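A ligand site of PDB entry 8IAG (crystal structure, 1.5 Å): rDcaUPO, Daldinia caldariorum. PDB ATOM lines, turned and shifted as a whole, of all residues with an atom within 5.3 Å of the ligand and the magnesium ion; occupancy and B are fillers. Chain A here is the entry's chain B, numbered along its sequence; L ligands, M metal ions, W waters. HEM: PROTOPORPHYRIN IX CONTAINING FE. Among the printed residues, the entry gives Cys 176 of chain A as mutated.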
ATOM      1  N   PRO A  31     -23.537  21.972  -1.930  1.00  0.00           N
ATOM      2  CA  PRO A  31     -22.396  21.687  -1.050  1.00  0.00           C
ATOM      3  C   PRO A  31     -21.771  20.314  -1.294  1.00  0.00           C
ATOM      4  O   PRO A  31     -20.774  19.991  -0.655  1.00  0.00           O
ATOM      5  CB  PRO A  31     -23.032  21.745   0.343  1.00  0.00           C
ATOM      6  CG  PRO A  31     -24.392  21.099   0.099  1.00  0.00           C
ATOM      7  CD  PRO A  31     -24.824  21.626  -1.303  1.00  0.00           C
ATOM      8  N   CYS A  32     -22.356  19.540  -2.206  1.00  0.00           N
ATOM      9  CA  CYS A  32     -21.846  18.212  -2.518  1.00  0.00           C
ATOM     10  C   CYS A  32     -20.910  18.240  -3.703  1.00  0.00           C
ATOM     11  O   CYS A  32     -21.344  18.554  -4.819  1.00  0.00           O
ATOM     12  CB  CYS A  32     -22.989  17.237  -2.798  1.00  0.00           C
ATOM     13  SG  CYS A  32     -22.331  15.586  -3.175  1.00  0.00           S
ATOM     14  N   PRO A  33     -19.617  17.928  -3.493  1.00  0.00           N
ATOM     15  CA  PRO A  33     -18.684  17.985  -4.632  1.00  0.00           C
ATOM     16  C   PRO A  33     -19.092  17.015  -5.738  1.00  0.00           C
ATOM     17  O   PRO A  33     -18.873  17.321  -6.919  1.00  0.00           O
ATOM     18  CB  PRO A  33     -17.337  17.559  -4.029  1.00  0.00           C
ATOM     19  CG  PRO A  33     -17.707  16.817  -2.745  1.00  0.00           C
ATOM     20  CD  PRO A  33     -18.988  17.451  -2.251  1.00  0.00           C
ATOM     21  N   MET A  34     -19.680  15.875  -5.370  1.00  0.00           N
ATOM     22  CA  MET A  34     -19.998  14.887  -6.402  1.00  0.00           C
ATOM     23  C   MET A  34     -21.238  15.284  -7.215  1.00  0.00           C
ATOM     24  O   MET A  34     -21.193  15.191  -8.440  1.00  0.00           O
ATOM     25  CB  MET A  34     -20.187  13.500  -5.798  1.00  0.00           C
ATOM     26  CG  MET A  34     -20.491  12.444  -6.893  1.00  0.00           C
ATOM     27  SD  MET A  34     -19.274  12.363  -8.256  1.00  0.00           S
ATOM     28  CE  MET A  34     -18.003  11.323  -7.508  1.00  0.00           C
ATOM     29  N   LEU A  35     -22.325  15.712  -6.570  1.00  0.00           N
ATOM     30  CA  LEU A  35     -23.485  16.110  -7.354  1.00  0.00           C
ATOM     31  C   LEU A  35     -23.170  17.312  -8.236  1.00  0.00           C
ATOM     32  O   LEU A  35     -23.657  17.405  -9.368  1.00  0.00           O
ATOM     33  CB  LEU A  35     -24.708  16.411  -6.471  1.00  0.00           C
ATOM     34  CG  LEU A  35     -25.259  15.233  -5.664  1.00  0.00           C
ATOM     35  CD1 LEU A  35     -26.636  15.612  -5.093  1.00  0.00           C
ATOM     36  CD2 LEU A  35     -25.347  13.964  -6.484  1.00  0.00           C
ATOM     37  N   THR A  56     -31.911  11.237 -10.634  1.00  0.00           N
ATOM     38  CA  THR A  56     -30.898  10.891  -9.645  1.00  0.00           C
ATOM     39  C   THR A  56     -30.354   9.470  -9.848  1.00  0.00           C
ATOM     40  O   THR A  56     -29.139   9.240  -9.864  1.00  0.00           O
ATOM     41  CB  THR A  56     -31.463  11.006  -8.220  1.00  0.00           C
ATOM     42  OG1 THR A  56     -31.877  12.365  -8.002  1.00  0.00           O
ATOM     43  CG2 THR A  56     -30.423  10.613  -7.179  1.00  0.00           C
ATOM     44  N   LEU A  60     -26.454   8.526 -10.865  1.00  0.00           N
ATOM     45  CA  LEU A  60     -25.565   7.787  -9.972  1.00  0.00           C
ATOM     46  C   LEU A  60     -25.194   6.414 -10.539  1.00  0.00           C
ATOM     47  O   LEU A  60     -24.089   5.923 -10.333  1.00  0.00           O
ATOM     48  CB  LEU A  60     -26.219   7.636  -8.596  1.00  0.00           C
ATOM     49  CG  LEU A  60     -26.453   8.979  -7.891  1.00  0.00           C
ATOM     50  CD1 LEU A  60     -27.177   8.758  -6.575  1.00  0.00           C
ATOM     51  CD2 LEU A  60     -25.121   9.680  -7.630  1.00  0.00           C
ATOM     52  N   LEU A  64     -21.336   6.368 -11.735  1.00  0.00           N
ATOM     53  CA  LEU A  64     -20.610   5.850 -10.574  1.00  0.00           C
ATOM     54  C   LEU A  64     -20.911   4.400 -10.227  1.00  0.00           C
ATOM     55  O   LEU A  64     -20.244   3.821  -9.367  1.00  0.00           O
ATOM     56  CB  LEU A  64     -20.892   6.708  -9.347  1.00  0.00           C
ATOM     57  CG  LEU A  64     -20.640   8.212  -9.475  1.00  0.00           C
ATOM     58  CD1 LEU A  64     -21.172   8.962  -8.254  1.00  0.00           C
ATOM     59  CD2 LEU A  64     -19.146   8.494  -9.717  1.00  0.00           C
ATOM     60  N   LEU A  66     -23.482   3.170  -8.550  1.00  0.00           N
ATOM     61  CA  LEU A  66     -24.084   2.890  -7.249  1.00  0.00           C
ATOM     62  C   LEU A  66     -25.270   1.957  -7.404  1.00  0.00           C
ATOM     63  O   LEU A  66     -25.926   1.964  -8.451  1.00  0.00           O
ATOM     64  CB  LEU A  66     -24.543   4.179  -6.567  1.00  0.00           C
ATOM     65  CG  LEU A  66     -23.497   5.281  -6.412  1.00  0.00           C
ATOM     66  CD1 LEU A  66     -24.005   6.340  -5.453  1.00  0.00           C
ATOM     67  CD2 LEU A  66     -22.156   4.706  -5.936  1.00  0.00           C
ATOM     68  N   SER A  71     -29.199   4.718  -4.392  1.00  0.00           N
ATOM     69  CA  SER A  71     -29.488   5.971  -5.091  1.00  0.00           C
ATOM     70  C   SER A  71     -30.884   6.498  -4.762  1.00  0.00           C
ATOM     71  O   SER A  71     -31.058   7.703  -4.567  1.00  0.00           O
ATOM     72  CB  SER A  71     -29.348   5.783  -6.606  1.00  0.00           C
ATOM     73  OG  SER A  71     -28.021   5.393  -6.930  1.00  0.00           O
ATOM     74  N   LEU A  74     -30.841   7.968  -1.296  1.00  0.00           N
ATOM     75  CA  LEU A  74     -30.173   9.263  -1.306  1.00  0.00           C
ATOM     76  C   LEU A  74     -31.114  10.342  -1.861  1.00  0.00           C
ATOM     77  O   LEU A  74     -31.175  11.453  -1.342  1.00  0.00           O
ATOM     78  CB  LEU A  74     -28.878   9.214  -2.120  1.00  0.00           C
ATOM     79  CG  LEU A  74     -27.768   8.376  -1.476  1.00  0.00           C
ATOM     80  CD1 LEU A  74     -26.559   8.287  -2.390  1.00  0.00           C
ATOM     81  CD2 LEU A  74     -27.382   8.984  -0.143  1.00  0.00           C
ATOM     82  N   HIS A  75     -31.877   9.998  -2.889  1.00  0.00           N
ATOM     83  CA  HIS A  75     -32.838  10.948  -3.438  1.00  0.00           C
ATOM     84  C   HIS A  75     -33.874  11.334  -2.380  1.00  0.00           C
ATOM     85  O   HIS A  75     -34.241  12.507  -2.260  1.00  0.00           O
ATOM     86  CB  HIS A  75     -33.540  10.369  -4.676  1.00  0.00           C
ATOM     87  CG  HIS A  75     -34.460  11.343  -5.322  1.00  0.00           C
ATOM     88  ND1 HIS A  75     -34.006  12.334  -6.176  1.00  0.00           N
ATOM     89  CD2 HIS A  75     -35.797  11.544  -5.195  1.00  0.00           C
ATOM     90  CE1 HIS A  75     -35.026  13.069  -6.573  1.00  0.00           C
ATOM     91  NE2 HIS A  75     -36.119  12.619  -5.984  1.00  0.00           N
ATOM     92  N   ALA A  78     -32.465  13.851  -0.233  1.00  0.00           N
ATOM     93  CA  ALA A  78     -32.327  15.119  -0.954  1.00  0.00           C
ATOM     94  C   ALA A  78     -33.628  15.906  -0.986  1.00  0.00           C
ATOM     95  O   ALA A  78     -33.626  17.125  -0.809  1.00  0.00           O
ATOM     96  CB  ALA A  78     -31.833  14.892  -2.378  1.00  0.00           C
ATOM     97  N   PHE A  90     -35.735  17.956  -6.247  1.00  0.00           N
ATOM     98  CA  PHE A  90     -34.942  18.982  -5.579  1.00  0.00           C
ATOM     99  C   PHE A  90     -34.021  19.645  -6.596  1.00  0.00           C
ATOM    100  O   PHE A  90     -33.818  19.112  -7.695  1.00  0.00           O
ATOM    101  CB  PHE A  90     -34.116  18.386  -4.426  1.00  0.00           C
ATOM    102  CG  PHE A  90     -32.973  17.516  -4.893  1.00  0.00           C
ATOM    103  CD1 PHE A  90     -33.197  16.212  -5.337  1.00  0.00           C
ATOM    104  CD2 PHE A  90     -31.663  18.013  -4.899  1.00  0.00           C
ATOM    105  CE1 PHE A  90     -32.150  15.412  -5.776  1.00  0.00           C
ATOM    106  CE2 PHE A  90     -30.596  17.210  -5.344  1.00  0.00           C
ATOM    107  CZ  PHE A  90     -30.838  15.906  -5.774  1.00  0.00           C
ATOM    108  N   LEU A  95     -29.812  21.843  -1.345  1.00  0.00           N
ATOM    109  CA  LEU A  95     -28.957  21.031  -0.496  1.00  0.00           C
ATOM    110  C   LEU A  95     -28.081  21.872   0.441  1.00  0.00           C
ATOM    111  O   LEU A  95     -27.577  21.349   1.446  1.00  0.00           O
ATOM    112  CB  LEU A  95     -28.066  20.136  -1.342  1.00  0.00           C
ATOM    113  CG  LEU A  95     -28.778  19.094  -2.208  1.00  0.00           C
ATOM    114  CD1 LEU A  95     -27.737  18.371  -3.034  1.00  0.00           C
ATOM    115  CD2 LEU A  95     -29.538  18.100  -1.361  1.00  0.00           C
ATOM    116  N   LEU A 101     -29.440  18.677   5.510  1.00  0.00           N
ATOM    117  CA  LEU A 101     -28.402  17.680   5.199  1.00  0.00           C
ATOM    118  C   LEU A 101     -26.999  18.287   5.275  1.00  0.00           C
ATOM    119  O   LEU A 101     -26.019  17.563   5.519  1.00  0.00           O
ATOM    120  CB  LEU A 101     -28.612  17.104   3.800  1.00  0.00           C
ATOM    121  CG  LEU A 101     -29.970  16.459   3.523  1.00  0.00           C
ATOM    122  CD1 LEU A 101     -29.964  15.819   2.143  1.00  0.00           C
ATOM    123  CD2 LEU A 101     -30.311  15.426   4.591  1.00  0.00           C
ATOM    124  N   GLU A 102     -26.888  19.588   5.024  1.00  0.00           N
ATOM    125  CA  GLU A 102     -25.616  20.290   5.177  1.00  0.00           C
ATOM    126  C   GLU A 102     -25.288  20.441   6.662  1.00  0.00           C
ATOM    127  O   GLU A 102     -26.190  20.636   7.482  1.00  0.00           O
ATOM    128  CB  GLU A 102     -25.706  21.652   4.485  1.00  0.00           C
ATOM    129  CG  GLU A 102     -24.368  22.399   4.346  1.00  0.00           C
ATOM    130  CD  GLU A 102     -23.904  23.033   5.642  1.00  0.00           C
ATOM    131  OE1 GLU A 102     -24.757  23.528   6.412  1.00  0.00           O
ATOM    132  OE2 GLU A 102     -22.693  23.019   5.904  1.00  0.00           O
ATOM    133  N   HIS A 103     -24.006  20.362   6.994  1.00  0.00           N
ATOM    134  CA  HIS A 103     -23.592  20.410   8.396  1.00  0.00           C
ATOM    135  C   HIS A 103     -22.198  21.023   8.554  1.00  0.00           C
ATOM    136  O   HIS A 103     -21.442  21.145   7.575  1.00  0.00           O
ATOM    137  CB  HIS A 103     -23.600  19.013   9.016  1.00  0.00           C
ATOM    138  CG  HIS A 103     -22.859  18.021   8.182  1.00  0.00           C
ATOM    139  ND1 HIS A 103     -21.477  17.937   8.184  1.00  0.00           N
ATOM    140  CD2 HIS A 103     -23.285  17.143   7.261  1.00  0.00           C
ATOM    141  CE1 HIS A 103     -21.100  17.024   7.311  1.00  0.00           C
ATOM    142  NE2 HIS A 103     -22.178  16.538   6.726  1.00  0.00           N
ATOM    143  N   ASP A 104     -21.880  21.375   9.794  1.00  0.00           N
ATOM    144  CA  ASP A 104     -20.562  21.865  10.135  1.00  0.00           C
ATOM    145  C   ASP A 104     -19.474  20.801   9.940  1.00  0.00           C
ATOM    146  O   ASP A 104     -19.759  19.623   9.737  1.00  0.00           O
ATOM    147  CB  ASP A 104     -20.543  22.351  11.589  1.00  0.00           C
ATOM    148  CG  ASP A 104     -21.417  23.576  11.819  1.00  0.00           C
ATOM    149  OD1 ASP A 104     -21.681  24.337  10.856  1.00  0.00           O
ATOM    150  OD2 ASP A 104     -21.826  23.776  12.985  1.00  0.00           O
ATOM    151  N   ALA A 105     -18.228  21.242  10.045  1.00  0.00           N
ATOM    152  CA  ALA A 105     -17.039  20.365   9.985  1.00  0.00           C
ATOM    153  C   ALA A 105     -16.922  19.649   8.640  1.00  0.00           C
ATOM    154  O   ALA A 105     -16.424  18.516   8.555  1.00  0.00           O
ATOM    155  CB  ALA A 105     -17.046  19.363  11.144  1.00  0.00           C
ATOM    156  N   SER A 106     -17.349  20.333   7.589  1.00  0.00           N
ATOM    157  CA  SER A 106     -17.143  19.849   6.234  1.00  0.00           C
ATOM    158  C   SER A 106     -15.652  19.839   5.893  1.00  0.00           C
ATOM    159  O   SER A 106     -14.867  20.609   6.456  1.00  0.00           O
ATOM    160  CB  SER A 106     -17.925  20.706   5.237  1.00  0.00           C
ATOM    161  OG  SER A 106     -19.321  20.527   5.426  1.00  0.00           O
ATOM    162  N   LEU A 107     -15.271  18.965   4.970  1.00  0.00           N
ATOM    163  CA  LEU A 107     -13.872  18.786   4.587  1.00  0.00           C
ATOM    164  C   LEU A 107     -13.369  19.904   3.677  1.00  0.00           C
ATOM    165  O   LEU A 107     -12.159  20.142   3.582  1.00  0.00           O
ATOM    166  CB  LEU A 107     -13.695  17.458   3.856  1.00  0.00           C
ATOM    167  CG  LEU A 107     -14.159  16.235   4.660  1.00  0.00           C
ATOM    168  CD1 LEU A 107     -13.952  14.975   3.841  1.00  0.00           C
ATOM    169  CD2 LEU A 107     -13.444  16.154   6.016  1.00  0.00           C
ATOM    170  N   SER A 108     -14.283  20.568   2.977  1.00  0.00           N
ATOM    171  CA  SER A 108     -13.868  21.507   1.932  1.00  0.00           C
ATOM    172  C   SER A 108     -14.703  22.777   1.888  1.00  0.00           C
ATOM    173  O   SER A 108     -14.509  23.600   0.993  1.00  0.00           O
ATOM    174  CB  SER A 108     -13.910  20.849   0.544  1.00  0.00           C
ATOM    175  OG  SER A 108     -15.248  20.557   0.157  1.00  0.00           O
ATOM    176  N   ARG A 109     -15.648  22.909   2.822  1.00  0.00           N
ATOM    177  CA  ARG A 109     -16.544  24.064   2.896  1.00  0.00           C
ATOM    178  C   ARG A 109     -16.379  24.742   4.258  1.00  0.00           C
ATOM    179  O   ARG A 109     -16.040  24.073   5.245  1.00  0.00           O
ATOM    180  CB  ARG A 109     -18.016  23.646   2.714  1.00  0.00           C
ATOM    181  CG  ARG A 109     -18.548  23.642   1.276  1.00  0.00           C
ATOM    182  CD  ARG A 109     -17.764  22.726   0.355  1.00  0.00           C
ATOM    183  NE  ARG A 109     -18.370  22.816  -0.986  1.00  0.00           N
ATOM    184  CZ  ARG A 109     -17.877  22.278  -2.100  1.00  0.00           C
ATOM    185  NH1 ARG A 109     -16.752  21.574  -2.075  1.00  0.00           N
ATOM    186  NH2 ARG A 109     -18.510  22.487  -3.265  1.00  0.00           N
ATOM    187  N   GLN A 110     -16.643  26.050   4.326  1.00  0.00           N
ATOM    188  CA  GLN A 110     -16.709  26.758   5.592  1.00  0.00           C
ATOM    189  C   GLN A 110     -17.969  26.343   6.360  1.00  0.00           C
ATOM    190  O   GLN A 110     -19.002  26.013   5.765  1.00  0.00           O
ATOM    191  CB  GLN A 110     -16.743  28.278   5.362  1.00  0.00           C
ATOM    192  CG  GLN A 110     -15.488  28.873   4.736  1.00  0.00           C
ATOM    193  CD  GLN A 110     -15.526  30.394   4.804  1.00  0.00           C
ATOM    194  OE1 GLN A 110     -15.958  31.059   3.867  1.00  0.00           O
ATOM    195  NE2 GLN A 110     -15.092  30.931   5.933  1.00  0.00           N
ATOM    196  N   PRO A 117     -21.853  28.068   3.174  1.00  0.00           N
ATOM    197  CA  PRO A 117     -21.396  26.673   3.296  1.00  0.00           C
ATOM    198  C   PRO A 117     -21.569  25.823   2.051  1.00  0.00           C
ATOM    199  O   PRO A 117     -21.503  24.588   2.140  1.00  0.00           O
ATOM    200  CB  PRO A 117     -22.284  26.146   4.429  1.00  0.00           C
ATOM    201  CG  PRO A 117     -23.577  26.861   4.199  1.00  0.00           C
ATOM    202  CD  PRO A 117     -23.184  28.265   3.760  1.00  0.00           C
ATOM    203  N   GLU A 173     -20.252  10.604   4.041  1.00  0.00           N
ATOM    204  CA  GLU A 173     -19.543  11.403   3.045  1.00  0.00           C
ATOM    205  C   GLU A 173     -18.099  10.926   2.904  1.00  0.00           C
ATOM    206  O   GLU A 173     -17.577  10.837   1.773  1.00  0.00           O
ATOM    207  CB  GLU A 173     -19.599  12.880   3.429  1.00  0.00           C
ATOM    208  CG  GLU A 173     -21.017  13.441   3.380  1.00  0.00           C
ATOM    209  CD  GLU A 173     -21.299  14.489   4.445  1.00  0.00           C
ATOM    210  OE1 GLU A 173     -20.355  14.999   5.066  1.00  0.00           O
ATOM    211  OE2 GLU A 173     -22.496  14.792   4.641  1.00  0.00           O
ATOM    212  N   THR A 174     -17.446  10.609   4.020  1.00  0.00           N
ATOM    213  CA  THR A 174     -16.060  10.150   3.963  1.00  0.00           C
ATOM    214  C   THR A 174     -15.946   8.770   3.300  1.00  0.00           C
ATOM    215  O   THR A 174     -15.077   8.550   2.454  1.00  0.00           O
ATOM    216  CB  THR A 174     -15.439  10.148   5.382  1.00  0.00           C
ATOM    217  OG1 THR A 174     -14.983  11.486   5.652  1.00  0.00           O
ATOM    218  CG2 THR A 174     -14.242   9.201   5.479  1.00  0.00           C
ATOM    219  N   CYS A 176     -17.920   7.690   1.114  1.00  0.00           N
ATOM    220  CA  CYS A 176     -18.216   7.920  -0.296  1.00  0.00           C
ATOM    221  C   CYS A 176     -16.983   8.396  -1.089  1.00  0.00           C
ATOM    222  O   CYS A 176     -16.721   7.846  -2.151  1.00  0.00           O
ATOM    223  CB  CYS A 176     -19.364   8.928  -0.443  1.00  0.00           C
ATOM    224  SG  CYS A 176     -20.994   8.143  -0.197  1.00  0.00           S
ATOM    225  N   TYR A 177     -16.200   9.365  -0.619  1.00  0.00           N
ATOM    226  CA  TYR A 177     -15.107   9.778  -1.498  1.00  0.00           C
ATOM    227  C   TYR A 177     -14.030   8.697  -1.610  1.00  0.00           C
ATOM    228  O   TYR A 177     -13.416   8.560  -2.679  1.00  0.00           O
ATOM    229  CB  TYR A 177     -14.506  11.138  -1.094  1.00  0.00           C
ATOM    230  CG  TYR A 177     -13.583  11.207   0.118  1.00  0.00           C
ATOM    231  CD1 TYR A 177     -12.260  10.756   0.056  1.00  0.00           C
ATOM    232  CD2 TYR A 177     -14.017  11.777   1.311  1.00  0.00           C
ATOM    233  CE1 TYR A 177     -11.413  10.851   1.162  1.00  0.00           C
ATOM    234  CE2 TYR A 177     -13.191  11.880   2.414  1.00  0.00           C
ATOM    235  CZ  TYR A 177     -11.880  11.421   2.350  1.00  0.00           C
ATOM    236  OH  TYR A 177     -11.057  11.514   3.449  1.00  0.00           O
ATOM    237  N   ILE A 180     -16.114   5.402  -3.629  1.00  0.00           N
ATOM    238  CA  ILE A 180     -16.768   5.619  -4.919  1.00  0.00           C
ATOM    239  C   ILE A 180     -15.747   6.109  -5.961  1.00  0.00           C
ATOM    240  O   ILE A 180     -15.837   5.747  -7.129  1.00  0.00           O
ATOM    241  CB  ILE A 180     -17.950   6.582  -4.770  1.00  0.00           C
ATOM    242  CG1 ILE A 180     -19.016   5.889  -3.924  1.00  0.00           C
ATOM    243  CG2 ILE A 180     -18.538   6.994  -6.134  1.00  0.00           C
ATOM    244  CD1 ILE A 180     -20.158   6.803  -3.517  1.00  0.00           C
ATOM    245  N   LEU A 181     -14.752   6.891  -5.523  1.00  0.00           N
ATOM    246  CA  LEU A 181     -13.638   7.229  -6.394  1.00  0.00           C
ATOM    247  C   LEU A 181     -12.556   6.145  -6.409  1.00  0.00           C
ATOM    248  O   LEU A 181     -11.789   6.045  -7.360  1.00  0.00           O
ATOM    249  CB  LEU A 181     -13.015   8.552  -5.965  1.00  0.00           C
ATOM    250  CG  LEU A 181     -13.844   9.813  -6.257  1.00  0.00           C
ATOM    251  CD1 LEU A 181     -13.120  11.007  -5.638  1.00  0.00           C
ATOM    252  CD2 LEU A 181     -14.034   9.987  -7.743  1.00  0.00           C
ATOM    253  N   LEU A 197     -11.356  15.751  -7.818  1.00  0.00           N
ATOM    254  CA  LEU A 197     -12.813  15.907  -7.720  1.00  0.00           C
ATOM    255  C   LEU A 197     -13.169  17.169  -6.948  1.00  0.00           C
ATOM    256  O   LEU A 197     -13.981  17.978  -7.398  1.00  0.00           O
ATOM    257  CB  LEU A 197     -13.444  14.695  -7.033  1.00  0.00           C
ATOM    258  CG  LEU A 197     -14.978  14.792  -6.988  1.00  0.00           C
ATOM    259  CD1 LEU A 197     -15.574  14.262  -8.291  1.00  0.00           C
ATOM    260  CD2 LEU A 197     -15.624  14.124  -5.763  1.00  0.00           C
ATOM    261  N   PHE A 198     -12.573  17.335  -5.763  1.00  0.00           N
ATOM    262  CA  PHE A 198     -12.910  18.509  -4.943  1.00  0.00           C
ATOM    263  C   PHE A 198     -12.501  19.830  -5.585  1.00  0.00           C
ATOM    264  O   PHE A 198     -13.256  20.804  -5.538  1.00  0.00           O
ATOM    265  CB  PHE A 198     -12.232  18.435  -3.577  1.00  0.00           C
ATOM    266  CG  PHE A 198     -12.962  17.588  -2.553  1.00  0.00           C
ATOM    267  CD1 PHE A 198     -12.704  16.227  -2.411  1.00  0.00           C
ATOM    268  CD2 PHE A 198     -13.840  18.191  -1.667  1.00  0.00           C
ATOM    269  CE1 PHE A 198     -13.377  15.480  -1.434  1.00  0.00           C
ATOM    270  CE2 PHE A 198     -14.498  17.473  -0.692  1.00  0.00           C
ATOM    271  CZ  PHE A 198     -14.261  16.120  -0.553  1.00  0.00           C
HETATM  272  CHA HEM L   1     -21.291  16.428   0.891  1.00  0.00           C
HETATM  273  CHB HEM L   1     -25.801  15.435  -0.519  1.00  0.00           C
HETATM  274  CHC HEM L   1     -24.103  11.946  -3.451  1.00  0.00           C
HETATM  275  CHD HEM L   1     -19.587  12.762  -1.830  1.00  0.00           C
HETATM  276  C1A HEM L   1     -22.637  16.501   0.712  1.00  0.00           C
HETATM  277  C2A HEM L   1     -23.513  17.461   1.339  1.00  0.00           C
HETATM  278  C3A HEM L   1     -24.776  17.169   0.959  1.00  0.00           C
HETATM  279  C4A HEM L   1     -24.719  16.037   0.047  1.00  0.00           C
HETATM  280  CMA HEM L   1     -26.060  17.908   1.377  1.00  0.00           C
HETATM  281  CAA HEM L   1     -23.018  18.574   2.289  1.00  0.00           C
HETATM  282  CBA HEM L   1     -22.676  17.993   3.664  1.00  0.00           C
HETATM  283  CGA HEM L   1     -21.681  18.931   4.278  1.00  0.00           C
HETATM  284  O1A HEM L   1     -20.468  18.726   4.042  1.00  0.00           O
HETATM  285  O2A HEM L   1     -22.061  19.904   4.989  1.00  0.00           O
HETATM  286  C1B HEM L   1     -25.725  14.393  -1.419  1.00  0.00           C
HETATM  287  C2B HEM L   1     -26.866  13.776  -2.080  1.00  0.00           C
HETATM  288  C3B HEM L   1     -26.394  12.825  -2.888  1.00  0.00           C
HETATM  289  C4B HEM L   1     -24.953  12.807  -2.782  1.00  0.00           C
HETATM  290  CMB HEM L   1     -28.333  14.182  -1.820  1.00  0.00           C
HETATM  291  CAB HEM L   1     -27.145  11.866  -3.833  1.00  0.00           C
HETATM  292  CBB HEM L   1     -28.373  12.100  -4.298  1.00  0.00           C
HETATM  293  C1C HEM L   1     -22.726  11.864  -3.271  1.00  0.00           C
HETATM  294  C2C HEM L   1     -21.850  10.917  -3.904  1.00  0.00           C
HETATM  295  C3C HEM L   1     -20.588  11.141  -3.486  1.00  0.00           C
HETATM  296  C4C HEM L   1     -20.649  12.234  -2.524  1.00  0.00           C
HETATM  297  CMC HEM L   1     -22.321   9.866  -4.921  1.00  0.00           C
HETATM  298  CAC HEM L   1     -19.346  10.340  -3.943  1.00  0.00           C
HETATM  299  CBC HEM L   1     -18.078  10.805  -3.889  1.00  0.00           C
HETATM  300  C1D HEM L   1     -19.676  13.771  -0.919  1.00  0.00           C
HETATM  301  C2D HEM L   1     -18.568  14.184  -0.095  1.00  0.00           C
HETATM  302  C3D HEM L   1     -19.086  15.313   0.741  1.00  0.00           C
HETATM  303  C4D HEM L   1     -20.463  15.468   0.361  1.00  0.00           C
HETATM  304  CMD HEM L   1     -17.143  13.617  -0.094  1.00  0.00           C
HETATM  305  CAD HEM L   1     -18.339  16.117   1.811  1.00  0.00           C
HETATM  306  CBD HEM L   1     -17.856  17.445   1.245  1.00  0.00           C
HETATM  307  CGD HEM L   1     -17.154  18.200   2.335  1.00  0.00           C
HETATM  308  O1D HEM L   1     -16.554  19.262   2.021  1.00  0.00           O
HETATM  309  O2D HEM L   1     -17.146  17.761   3.505  1.00  0.00           O
HETATM  310  NA  HEM L   1     -23.395  15.646  -0.089  1.00  0.00           N
HETATM  311  NB  HEM L   1     -24.574  13.774  -1.859  1.00  0.00           N
HETATM  312  NC  HEM L   1     -21.958  12.646  -2.425  1.00  0.00           N
HETATM  313  ND  HEM L   1     -20.796  14.539  -0.610  1.00  0.00           N
HETATM  314 FE   HEM L   1     -22.676  14.197  -1.308  1.00  0.00          FE
HETATM  315 MG    MG M   1     -21.063  21.773   5.572  1.00  0.00          MG
HETATM  316  O   HOH W   1     -19.763  20.544   1.876  1.00  0.00           O
HETATM  317  O   HOH W   2     -21.015  22.345   3.543  1.00  0.00           O
HETATM  318  O   HOH W   3     -17.901  15.807   5.295  1.00  0.00           O
HETATM  319  O   HOH W   4     -19.842  23.348   6.197  1.00  0.00           O
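An oxygen (O2A) of the ligand sits close to the backbone NH (N) of His 103, 2.8 Å away.
The backbone NH of Ser 108 lies within hydrogen-bond range of an oxygen (O1D) of the ligand, 2.8 Å away.
SG of Cys 32 binds FE of the ligand (2.4 Å).
N of Leu 107 is in hydrogen-bond range of O2D of the ligand.
The side-chain hydroxyl of Ser 108 sits at hydrogen-bond distance from an oxygen (O1D) of the ligand.
The side-chain hydroxyl (OG1) of Thr 56 lies within hydrogen-bond range of a ring nitrogen (ND1) of His 75 (2.8 Å).
The backbone NH (N) of Leu 35 lies close to the side-chain sulfur (SG) of Cys 32 (3.4 Å).
OG of Ser 108 sits at hydrogen-bond distance from NH1 of Arg 109 (2.9 Å).
The side-chain sulfur (SG) of Cys 32 sits close to the backbone NH (N) of Met 34 (3.5 Å).
The side-chain carboxylate (OE2) of Glu 173 lies within hydrogen-bond range of a ring nitrogen (NE2) of His 103, 2.7 Å away.
The backbone NH (N) of Leu 66 sits at hydrogen-bond distance from the backbone carbonyl oxygen (O) of Leu 60 (3.3 Å).
CG of Pro 31 touches CAA of the ligand (3.6 Å).
CD of Pro 33 touches C4D of the ligand, at 3.6 Å.
Met 34 touches the ligand (CB to C3C, 3.3 Å).
Leu 35 touches the ligand.
CG2 of Thr 56 touches CBB of the ligand, at 3.8 Å.
Leu 60 touches the ligand (CD2 to CMC, 3.9 Å).
Leu 64 touches the ligand (CD1 to CMC, 3.6 Å).
Leu 66 touches the ligand.
Leu 74 touches the ligand.
Ala 78 touches the ligand.
Leu 95 touches the ligand.
CB of Leu 101 touches CMA of the ligand, 3.6 Å away.
Arg 109 touches the ligand.
OE2 of Glu 173 touches CBA of the ligand, at 3.4 Å.
Cys 176 touches the ligand.
CB of Tyr 177 touches CMD of the ligand, 3.8 Å away.
Ile 180 touches the ligand.
CZ of Phe 198 touches CMD of the ligand, 3.8 Å away.
Hydrophobic or aromatic side chains that line the ligand: Pro 31, Pro 33, Met 34, Leu 35, Leu 60, Leu 64, Leu 66, Leu 74, Ala 78, Leu 101, His 103, Leu 107, Tyr 177, Ile 180 and Phe 198.
Within 4 Å of the ligand: Pro 31, Cys 32, Pro 33, Met 34, Leu 35, Thr 56, Leu 60, Leu 64, Leu 66, Leu 74, Ala 78, Leu 95, Leu 101, Glu 102, His 103, Ser 106, Leu 107, Ser 108, Arg 109, Glu 173, Cys 176, Tyr 177, Ile 180 and Phe 198.
The nearest printed residue that does not touch the ligand is His 75 (4.3 Å).
Three residues have an atom within 4 Å of the magnesium ion: Glu 102, His 103 and Ser 106.
The nearest printed residue that does not touch the magnesium ion is Asp 104 (4.3 Å).
The magnesium ion is bound by the side-chain carboxylate (OE2) of Glu 102, 2.1 Å away.
Water W4 binds the magnesium ion (2.1 Å).
The magnesium ion is bound by water W2 (2.1 Å).
The backbone carbonyl oxygen (O) of His 103 is bound to the magnesium ion, 2.1 Å away.
The magnesium ion is bound by the side-chain hydroxyl (OG) of Ser 106, 2.1 Å away.
An oxygen (O2A) of the ligand is bound to the magnesium ion.
Water W3 lies within hydrogen-bond range of OE1 of Glu 173 and O2D of the ligand.
Water W1 lies within hydrogen-bond range of O of Pro 31 and O1A of the ligand.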
